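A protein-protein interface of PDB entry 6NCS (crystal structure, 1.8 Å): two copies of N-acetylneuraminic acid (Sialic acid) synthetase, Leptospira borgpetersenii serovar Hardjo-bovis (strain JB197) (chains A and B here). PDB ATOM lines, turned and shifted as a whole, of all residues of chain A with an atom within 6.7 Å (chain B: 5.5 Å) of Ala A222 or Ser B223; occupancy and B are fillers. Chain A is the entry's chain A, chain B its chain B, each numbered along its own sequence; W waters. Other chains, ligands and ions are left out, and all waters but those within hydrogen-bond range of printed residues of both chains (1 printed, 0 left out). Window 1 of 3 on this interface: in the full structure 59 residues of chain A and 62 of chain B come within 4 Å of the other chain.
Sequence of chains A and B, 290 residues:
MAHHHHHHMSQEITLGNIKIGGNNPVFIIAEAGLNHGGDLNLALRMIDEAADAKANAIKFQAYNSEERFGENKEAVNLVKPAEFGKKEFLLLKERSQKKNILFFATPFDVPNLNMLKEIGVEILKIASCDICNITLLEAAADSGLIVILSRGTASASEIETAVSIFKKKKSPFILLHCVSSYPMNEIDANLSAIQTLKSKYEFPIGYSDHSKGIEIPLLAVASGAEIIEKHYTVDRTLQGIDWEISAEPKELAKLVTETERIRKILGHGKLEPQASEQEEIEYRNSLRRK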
ATOM      1  N   GLN A 195     -14.705   4.963  -7.988  1.00  0.00           N
ATOM      2  CA  GLN A 195     -14.298   4.975  -9.387  1.00  0.00           C
ATOM      3  C   GLN A 195     -12.782   4.969  -9.527  1.00  0.00           C
ATOM      4  O   GLN A 195     -12.248   4.375 -10.470  1.00  0.00           O
ATOM      5  CB  GLN A 195     -14.893   6.186 -10.107  1.00  0.00           C
ATOM      6  CG  GLN A 195     -16.314   5.994 -10.528  1.00  0.00           C
ATOM      7  CD  GLN A 195     -16.472   4.888 -11.547  1.00  0.00           C
ATOM      8  OE1 GLN A 195     -15.581   4.652 -12.370  1.00  0.00           O
ATOM      9  NE2 GLN A 195     -17.603   4.195 -11.491  1.00  0.00           N
ATOM     10  N   PRO A 217     -25.004   4.850   1.135  1.00  0.00           N
ATOM     11  CA  PRO A 217     -24.821   3.620   0.340  1.00  0.00           C
ATOM     12  C   PRO A 217     -25.575   3.615  -0.996  1.00  0.00           C
ATOM     13  O   PRO A 217     -25.064   3.068  -1.980  1.00  0.00           O
ATOM     14  CB  PRO A 217     -25.307   2.503   1.287  1.00  0.00           C
ATOM     15  CG  PRO A 217     -25.887   3.159   2.479  1.00  0.00           C
ATOM     16  CD  PRO A 217     -25.348   4.564   2.539  1.00  0.00           C
ATOM     17  N   LEU A 218     -26.758   4.217  -1.076  1.00  0.00           N
ATOM     18  CA  LEU A 218     -27.441   4.299  -2.370  1.00  0.00           C
ATOM     19  C   LEU A 218     -26.673   5.189  -3.340  1.00  0.00           C
ATOM     20  O   LEU A 218     -26.540   4.857  -4.529  1.00  0.00           O
ATOM     21  CB  LEU A 218     -28.869   4.820  -2.183  1.00  0.00           C
ATOM     22  CG  LEU A 218     -29.742   3.803  -1.421  1.00  0.00           C
ATOM     23  CD1 LEU A 218     -31.086   4.407  -1.108  1.00  0.00           C
ATOM     24  CD2 LEU A 218     -29.915   2.559  -2.284  1.00  0.00           C
ATOM     25  N   LEU A 219     -26.189   6.339  -2.863  1.00  0.00           N
ATOM     26  CA  LEU A 219     -25.320   7.152  -3.704  1.00  0.00           C
ATOM     27  C   LEU A 219     -24.073   6.375  -4.106  1.00  0.00           C
ATOM     28  O   LEU A 219     -23.570   6.541  -5.223  1.00  0.00           O
ATOM     29  CB  LEU A 219     -24.945   8.457  -2.987  1.00  0.00           C
ATOM     30  CG  LEU A 219     -26.106   9.445  -2.808  1.00  0.00           C
ATOM     31  CD1 LEU A 219     -25.727  10.586  -1.898  1.00  0.00           C
ATOM     32  CD2 LEU A 219     -26.555   9.961  -4.171  1.00  0.00           C
ATOM     33  N   ALA A 220     -23.583   5.493  -3.230  1.00  0.00           N
ATOM     34  CA  ALA A 220     -22.406   4.706  -3.585  1.00  0.00           C
ATOM     35  C   ALA A 220     -22.701   3.761  -4.737  1.00  0.00           C
ATOM     36  O   ALA A 220     -21.859   3.581  -5.626  1.00  0.00           O
ATOM     37  CB  ALA A 220     -21.894   3.927  -2.366  1.00  0.00           C
ATOM     38  N   VAL A 221     -23.903   3.176  -4.760  1.00  0.00           N
ATOM     39  CA  VAL A 221     -24.333   2.379  -5.913  1.00  0.00           C
ATOM     40  C   VAL A 221     -24.338   3.223  -7.179  1.00  0.00           C
ATOM     41  O   VAL A 221     -23.837   2.795  -8.223  1.00  0.00           O
ATOM     42  CB  VAL A 221     -25.716   1.746  -5.659  1.00  0.00           C
ATOM     43  CG1 VAL A 221     -26.226   1.068  -6.923  1.00  0.00           C
ATOM     44  CG2 VAL A 221     -25.648   0.748  -4.513  1.00  0.00           C
ATOM     45  N   ALA A 222     -24.909   4.435  -7.115  1.00  0.00           N
ATOM     46  CA  ALA A 222     -24.890   5.291  -8.299  1.00  0.00           C
ATOM     47  C   ALA A 222     -23.467   5.644  -8.716  1.00  0.00           C
ATOM     48  O   ALA A 222     -23.199   5.848  -9.908  1.00  0.00           O
ATOM     49  CB  ALA A 222     -25.701   6.571  -8.061  1.00  0.00           C
ATOM     50  N   SER A 223     -22.539   5.704  -7.770  1.00  0.00           N
ATOM     51  CA  SER A 223     -21.162   6.026  -8.103  1.00  0.00           C
ATOM     52  C   SER A 223     -20.343   4.794  -8.486  1.00  0.00           C
ATOM     53  O   SER A 223     -19.124   4.908  -8.654  1.00  0.00           O
ATOM     54  CB  SER A 223     -20.493   6.768  -6.947  1.00  0.00           C
ATOM     55  OG  SER A 223     -20.174   5.880  -5.897  1.00  0.00           O
ATOM     56  N   GLY A 224     -20.972   3.631  -8.622  1.00  0.00           N
ATOM     57  CA  GLY A 224     -20.296   2.456  -9.163  1.00  0.00           C
ATOM     58  C   GLY A 224     -20.126   1.272  -8.229  1.00  0.00           C
ATOM     59  O   GLY A 224     -19.568   0.255  -8.665  1.00  0.00           O
ATOM     60  N   ALA A 225     -20.560   1.329  -6.970  1.00  0.00           N
ATOM     61  CA  ALA A 225     -20.345   0.202  -6.057  1.00  0.00           C
ATOM     62  C   ALA A 225     -21.055  -1.057  -6.543  1.00  0.00           C
ATOM     63  O   ALA A 225     -22.220  -1.014  -6.945  1.00  0.00           O
ATOM     64  CB  ALA A 225     -20.828   0.564  -4.657  1.00  0.00           C
ATOM     65  N   ILE A 262     -31.808   1.827  -8.623  1.00  0.00           N
ATOM     66  CA  ILE A 262     -30.703   2.639  -9.133  1.00  0.00           C
ATOM     67  C   ILE A 262     -29.899   1.858 -10.170  1.00  0.00           C
ATOM     68  O   ILE A 262     -29.457   2.420 -11.178  1.00  0.00           O
ATOM     69  CB  ILE A 262     -29.822   3.136  -7.971  1.00  0.00           C
ATOM     70  CG1 ILE A 262     -30.596   4.149  -7.131  1.00  0.00           C
ATOM     71  CG2 ILE A 262     -28.529   3.771  -8.487  1.00  0.00           C
ATOM     72  CD1 ILE A 262     -29.932   4.478  -5.767  1.00  0.00           C
ATOM     73  N   LEU A 266     -28.856   3.089 -13.842  1.00  0.00           N
ATOM     74  CA  LEU A 266     -27.508   3.078 -14.402  1.00  0.00           C
ATOM     75  C   LEU A 266     -27.473   2.379 -15.751  1.00  0.00           C
ATOM     76  O   LEU A 266     -26.744   2.806 -16.658  1.00  0.00           O
ATOM     77  CB  LEU A 266     -26.527   2.395 -13.446  1.00  0.00           C
ATOM     78  CG  LEU A 266     -26.209   3.149 -12.158  1.00  0.00           C
ATOM     79  CD1 LEU A 266     -25.433   2.265 -11.207  1.00  0.00           C
ATOM     80  CD2 LEU A 266     -25.389   4.388 -12.492  1.00  0.00           C
ATOM     81  N   LEU B 191     -27.457   5.829 -17.058  1.00  0.00           N
ATOM     82  CA  LEU B 191     -26.502   6.783 -16.514  1.00  0.00           C
ATOM     83  C   LEU B 191     -25.071   6.258 -16.496  1.00  0.00           C
ATOM     84  O   LEU B 191     -24.135   7.062 -16.411  1.00  0.00           O
ATOM     85  CB  LEU B 191     -26.904   7.199 -15.097  1.00  0.00           C
ATOM     86  CG  LEU B 191     -28.213   7.989 -15.015  1.00  0.00           C
ATOM     87  CD1 LEU B 191     -28.367   8.516 -13.585  1.00  0.00           C
ATOM     88  CD2 LEU B 191     -28.302   9.127 -16.051  1.00  0.00           C
ATOM     89  N   SER B 192     -24.868   4.946 -16.546  1.00  0.00           N
ATOM     90  CA  SER B 192     -23.490   4.478 -16.561  1.00  0.00           C
ATOM     91  C   SER B 192     -22.780   4.828 -17.861  1.00  0.00           C
ATOM     92  O   SER B 192     -21.550   4.719 -17.914  1.00  0.00           O
ATOM     93  CB  SER B 192     -23.425   2.972 -16.308  1.00  0.00           C
ATOM     94  OG  SER B 192     -24.282   2.270 -17.181  1.00  0.00           O
ATOM     95  N   ILE B 194     -22.253   7.701 -18.677  1.00  0.00           N
ATOM     96  CA  ILE B 194     -21.420   8.838 -18.302  1.00  0.00           C
ATOM     97  C   ILE B 194     -20.003   8.372 -17.999  1.00  0.00           C
ATOM     98  O   ILE B 194     -19.023   8.942 -18.496  1.00  0.00           O
ATOM     99  CB  ILE B 194     -22.051   9.588 -17.111  1.00  0.00           C
ATOM    100  CG1 ILE B 194     -23.367  10.237 -17.545  1.00  0.00           C
ATOM    101  CG2 ILE B 194     -21.091  10.651 -16.565  1.00  0.00           C
ATOM    102  CD1 ILE B 194     -24.199  10.790 -16.385  1.00  0.00           C
ATOM    103  N   GLN B 195     -19.872   7.310 -17.198  1.00  0.00           N
ATOM    104  CA  GLN B 195     -18.550   6.756 -16.923  1.00  0.00           C
ATOM    105  C   GLN B 195     -17.908   6.173 -18.175  1.00  0.00           C
ATOM    106  O   GLN B 195     -16.680   6.216 -18.319  1.00  0.00           O
ATOM    107  CB  GLN B 195     -18.629   5.681 -15.836  1.00  0.00           C
ATOM    108  CG  GLN B 195     -18.518   6.199 -14.417  1.00  0.00           C
ATOM    109  CD  GLN B 195     -17.355   7.169 -14.192  1.00  0.00           C
ATOM    110  OE1 GLN B 195     -16.238   6.968 -14.674  1.00  0.00           O
ATOM    111  NE2 GLN B 195     -17.627   8.230 -13.444  1.00  0.00           N
ATOM    112  N   LYS B 198     -16.491   9.068 -19.867  1.00  0.00           N
ATOM    113  CA  LYS B 198     -15.334   9.626 -19.173  1.00  0.00           C
ATOM    114  C   LYS B 198     -14.105   8.749 -19.374  1.00  0.00           C
ATOM    115  O   LYS B 198     -12.978   9.259 -19.445  1.00  0.00           O
ATOM    116  CB  LYS B 198     -15.642   9.816 -17.687  1.00  0.00           C
ATOM    117  CG  LYS B 198     -16.686  10.875 -17.392  1.00  0.00           C
ATOM    118  CD  LYS B 198     -16.984  10.968 -15.900  1.00  0.00           C
ATOM    119  CE  LYS B 198     -16.237  12.127 -15.252  1.00  0.00           C
ATOM    120  NZ  LYS B 198     -16.542  12.240 -13.798  1.00  0.00           N
ATOM    121  N   LEU B 218     -29.768  14.291 -10.315  1.00  0.00           N
ATOM    122  CA  LEU B 218     -28.927  14.166  -9.127  1.00  0.00           C
ATOM    123  C   LEU B 218     -28.190  12.832  -9.103  1.00  0.00           C
ATOM    124  O   LEU B 218     -27.010  12.784  -8.733  1.00  0.00           O
ATOM    125  CB  LEU B 218     -29.760  14.362  -7.860  1.00  0.00           C
ATOM    126  CG  LEU B 218     -30.307  15.786  -7.706  1.00  0.00           C
ATOM    127  CD1 LEU B 218     -31.289  15.860  -6.547  1.00  0.00           C
ATOM    128  CD2 LEU B 218     -29.152  16.795  -7.490  1.00  0.00           C
ATOM    129  N   LEU B 219     -28.857  11.731  -9.482  1.00  0.00           N
ATOM    130  CA  LEU B 219     -28.129  10.479  -9.646  1.00  0.00           C
ATOM    131  C   LEU B 219     -27.056  10.591 -10.720  1.00  0.00           C
ATOM    132  O   LEU B 219     -26.016   9.927 -10.632  1.00  0.00           O
ATOM    133  CB  LEU B 219     -29.092   9.338  -9.982  1.00  0.00           C
ATOM    134  CG  LEU B 219     -30.019   8.940  -8.836  1.00  0.00           C
ATOM    135  CD1 LEU B 219     -31.111   7.998  -9.343  1.00  0.00           C
ATOM    136  CD2 LEU B 219     -29.229   8.265  -7.723  1.00  0.00           C
ATOM    137  N   ALA B 220     -27.289  11.410 -11.747  1.00  0.00           N
ATOM    138  CA  ALA B 220     -26.275  11.581 -12.782  1.00  0.00           C
ATOM    139  C   ALA B 220     -25.026  12.261 -12.226  1.00  0.00           C
ATOM    140  O   ALA B 220     -23.902  11.901 -12.596  1.00  0.00           O
ATOM    141  CB  ALA B 220     -26.860  12.377 -13.951  1.00  0.00           C
ATOM    142  N   VAL B 221     -25.207  13.242 -11.338  1.00  0.00           N
ATOM    143  CA  VAL B 221     -24.073  13.829 -10.619  1.00  0.00           C
ATOM    144  C   VAL B 221     -23.320  12.747  -9.855  1.00  0.00           C
ATOM    145  O   VAL B 221     -22.085  12.665  -9.909  1.00  0.00           O
ATOM    146  CB  VAL B 221     -24.556  14.948  -9.678  1.00  0.00           C
ATOM    147  CG1 VAL B 221     -23.418  15.466  -8.793  1.00  0.00           C
ATOM    148  CG2 VAL B 221     -25.158  16.081 -10.488  1.00  0.00           C
ATOM    149  N   ALA B 222     -24.053  11.890  -9.132  1.00  0.00           N
ATOM    150  CA  ALA B 222     -23.374  10.848  -8.364  1.00  0.00           C
ATOM    151  C   ALA B 222     -22.645   9.879  -9.285  1.00  0.00           C
ATOM    152  O   ALA B 222     -21.618   9.309  -8.901  1.00  0.00           O
ATOM    153  CB  ALA B 222     -24.367  10.090  -7.468  1.00  0.00           C
ATOM    154  N   SER B 223     -23.141   9.702 -10.506  1.00  0.00           N
ATOM    155  CA  SER B 223     -22.493   8.803 -11.451  1.00  0.00           C
ATOM    156  C   SER B 223     -21.407   9.489 -12.272  1.00  0.00           C
ATOM    157  O   SER B 223     -20.859   8.867 -13.194  1.00  0.00           O
ATOM    158  CB  SER B 223     -23.531   8.165 -12.383  1.00  0.00           C
ATOM    159  OG  SER B 223     -23.955   9.075 -13.376  1.00  0.00           O
ATOM    160  N   GLY B 224     -21.077  10.739 -11.959  1.00  0.00           N
ATOM    161  CA  GLY B 224     -19.919  11.384 -12.541  1.00  0.00           C
ATOM    162  C   GLY B 224     -20.199  12.602 -13.396  1.00  0.00           C
ATOM    163  O   GLY B 224     -19.237  13.193 -13.904  1.00  0.00           O
ATOM    164  N   ALA B 225     -21.446  13.026 -13.594  1.00  0.00           N
ATOM    165  CA  ALA B 225     -21.691  14.152 -14.495  1.00  0.00           C
ATOM    166  C   ALA B 225     -21.053  15.435 -13.970  1.00  0.00           C
ATOM    167  O   ALA B 225     -21.148  15.765 -12.783  1.00  0.00           O
ATOM    168  CB  ALA B 225     -23.188  14.368 -14.691  1.00  0.00           C
HETATM  169  O   HOH W   1     -19.154   6.812 -11.444  1.00  0.00           O
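The side-chain hydroxyl (OG) of Ser B192 sits at hydrogen-bond distance from the backbone carbonyl oxygen (O) of Leu A266, at 2.6 Å.
OE1 of Gln A195 lies close to OE1 of Gln B195 (3.3 Å).
The backbone carbonyl oxygen (O) of Leu A266 sits at hydrogen-bond distance from the backbone NH (N) of Leu B191, 3.1 Å away.
The side-chain hydroxyl (OG) of Ser A223 lies within hydrogen-bond range of the backbone carbonyl oxygen (O) of Ala A220 (2.9 Å).
NE2 of Gln B195 sits at hydrogen-bond distance from O of Ser B223, at 3.3 Å.
The backbone carbonyl oxygen of Ser A223 is in hydrogen-bond range of the side-chain amide nitrogen of Gln A195 (3.3 Å).
The backbone carbonyl oxygen (O) of Ala B220 lies within hydrogen-bond range of the side-chain hydroxyl (OG) of Ser B223 (2.9 Å).
Among the printed residues, merely in contact across the chains: Leu A219 with Ala B222 (3.96 Å), Ala A222 with Leu B219 (3.9 Å), Ala A222 with Ala B222 (3.8 Å), Ala A222 with Ser B223 (3.4 Å) and Ser A223 with Ala B222 (3.4 Å).
Printed residues of chain B within 4 Å of Leu A219: Ala B222 (3.96 Å).
Of the printed residues of chain B, Ala A222 touches Leu B219 (3.9 Å), Ala B222 (3.8 Å) and Ser B223 (3.4 Å).
Of the printed residues of chain B, Ser A223 touches Ala B222 (3.4 Å).
Of the printed residues of chain B, Leu A266 touches Leu B191 (3.1 Å) and Ser B192 (2.6 Å).
Printed residues of chain A within 4 Å of Ser B192: Leu A266 (2.6 Å).
Of the printed residues of chain A, Ala B222 touches Leu A219, Ala A222 and Ser A223.
Of the printed residues of chain A, Ser B223 touches Ala A222.
The nearest printed residue of chain B that does not touch Ala A222 is Gly B224 (5.7 Å).
Of the 12 printed residues of chain A, 5 touch a printed residue of chain B.
Along chain A the printed residues that touch a printed residue of chain B span positions 195 to 266.
Printed residues of chain B that touch a printed residue of chain A: Leu B191, Ser B192, Gln B195, Leu B219, Ala B222 and Ser B223.
Among the printed residues, no Asp or Glu carboxylate lies within 4 Å of a Lys or Arg side-chain nitrogen of the other chain.
Gln A195 touches its own counterpart, Gln B195.
Leu A219 touches Ala B222, and with the chains exchanged Ala A222 touches Leu B219.
Ala B222 touches its own counterpart, Ala A222.
Ala A222 touches Ser B223, and with the chains exchanged Ser A223 touches Ala B222.
Water W1 lies within hydrogen-bond range of NE2 of Gln B195, NE2 of Gln A195, O of Ser B223 and O of Ser A223.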
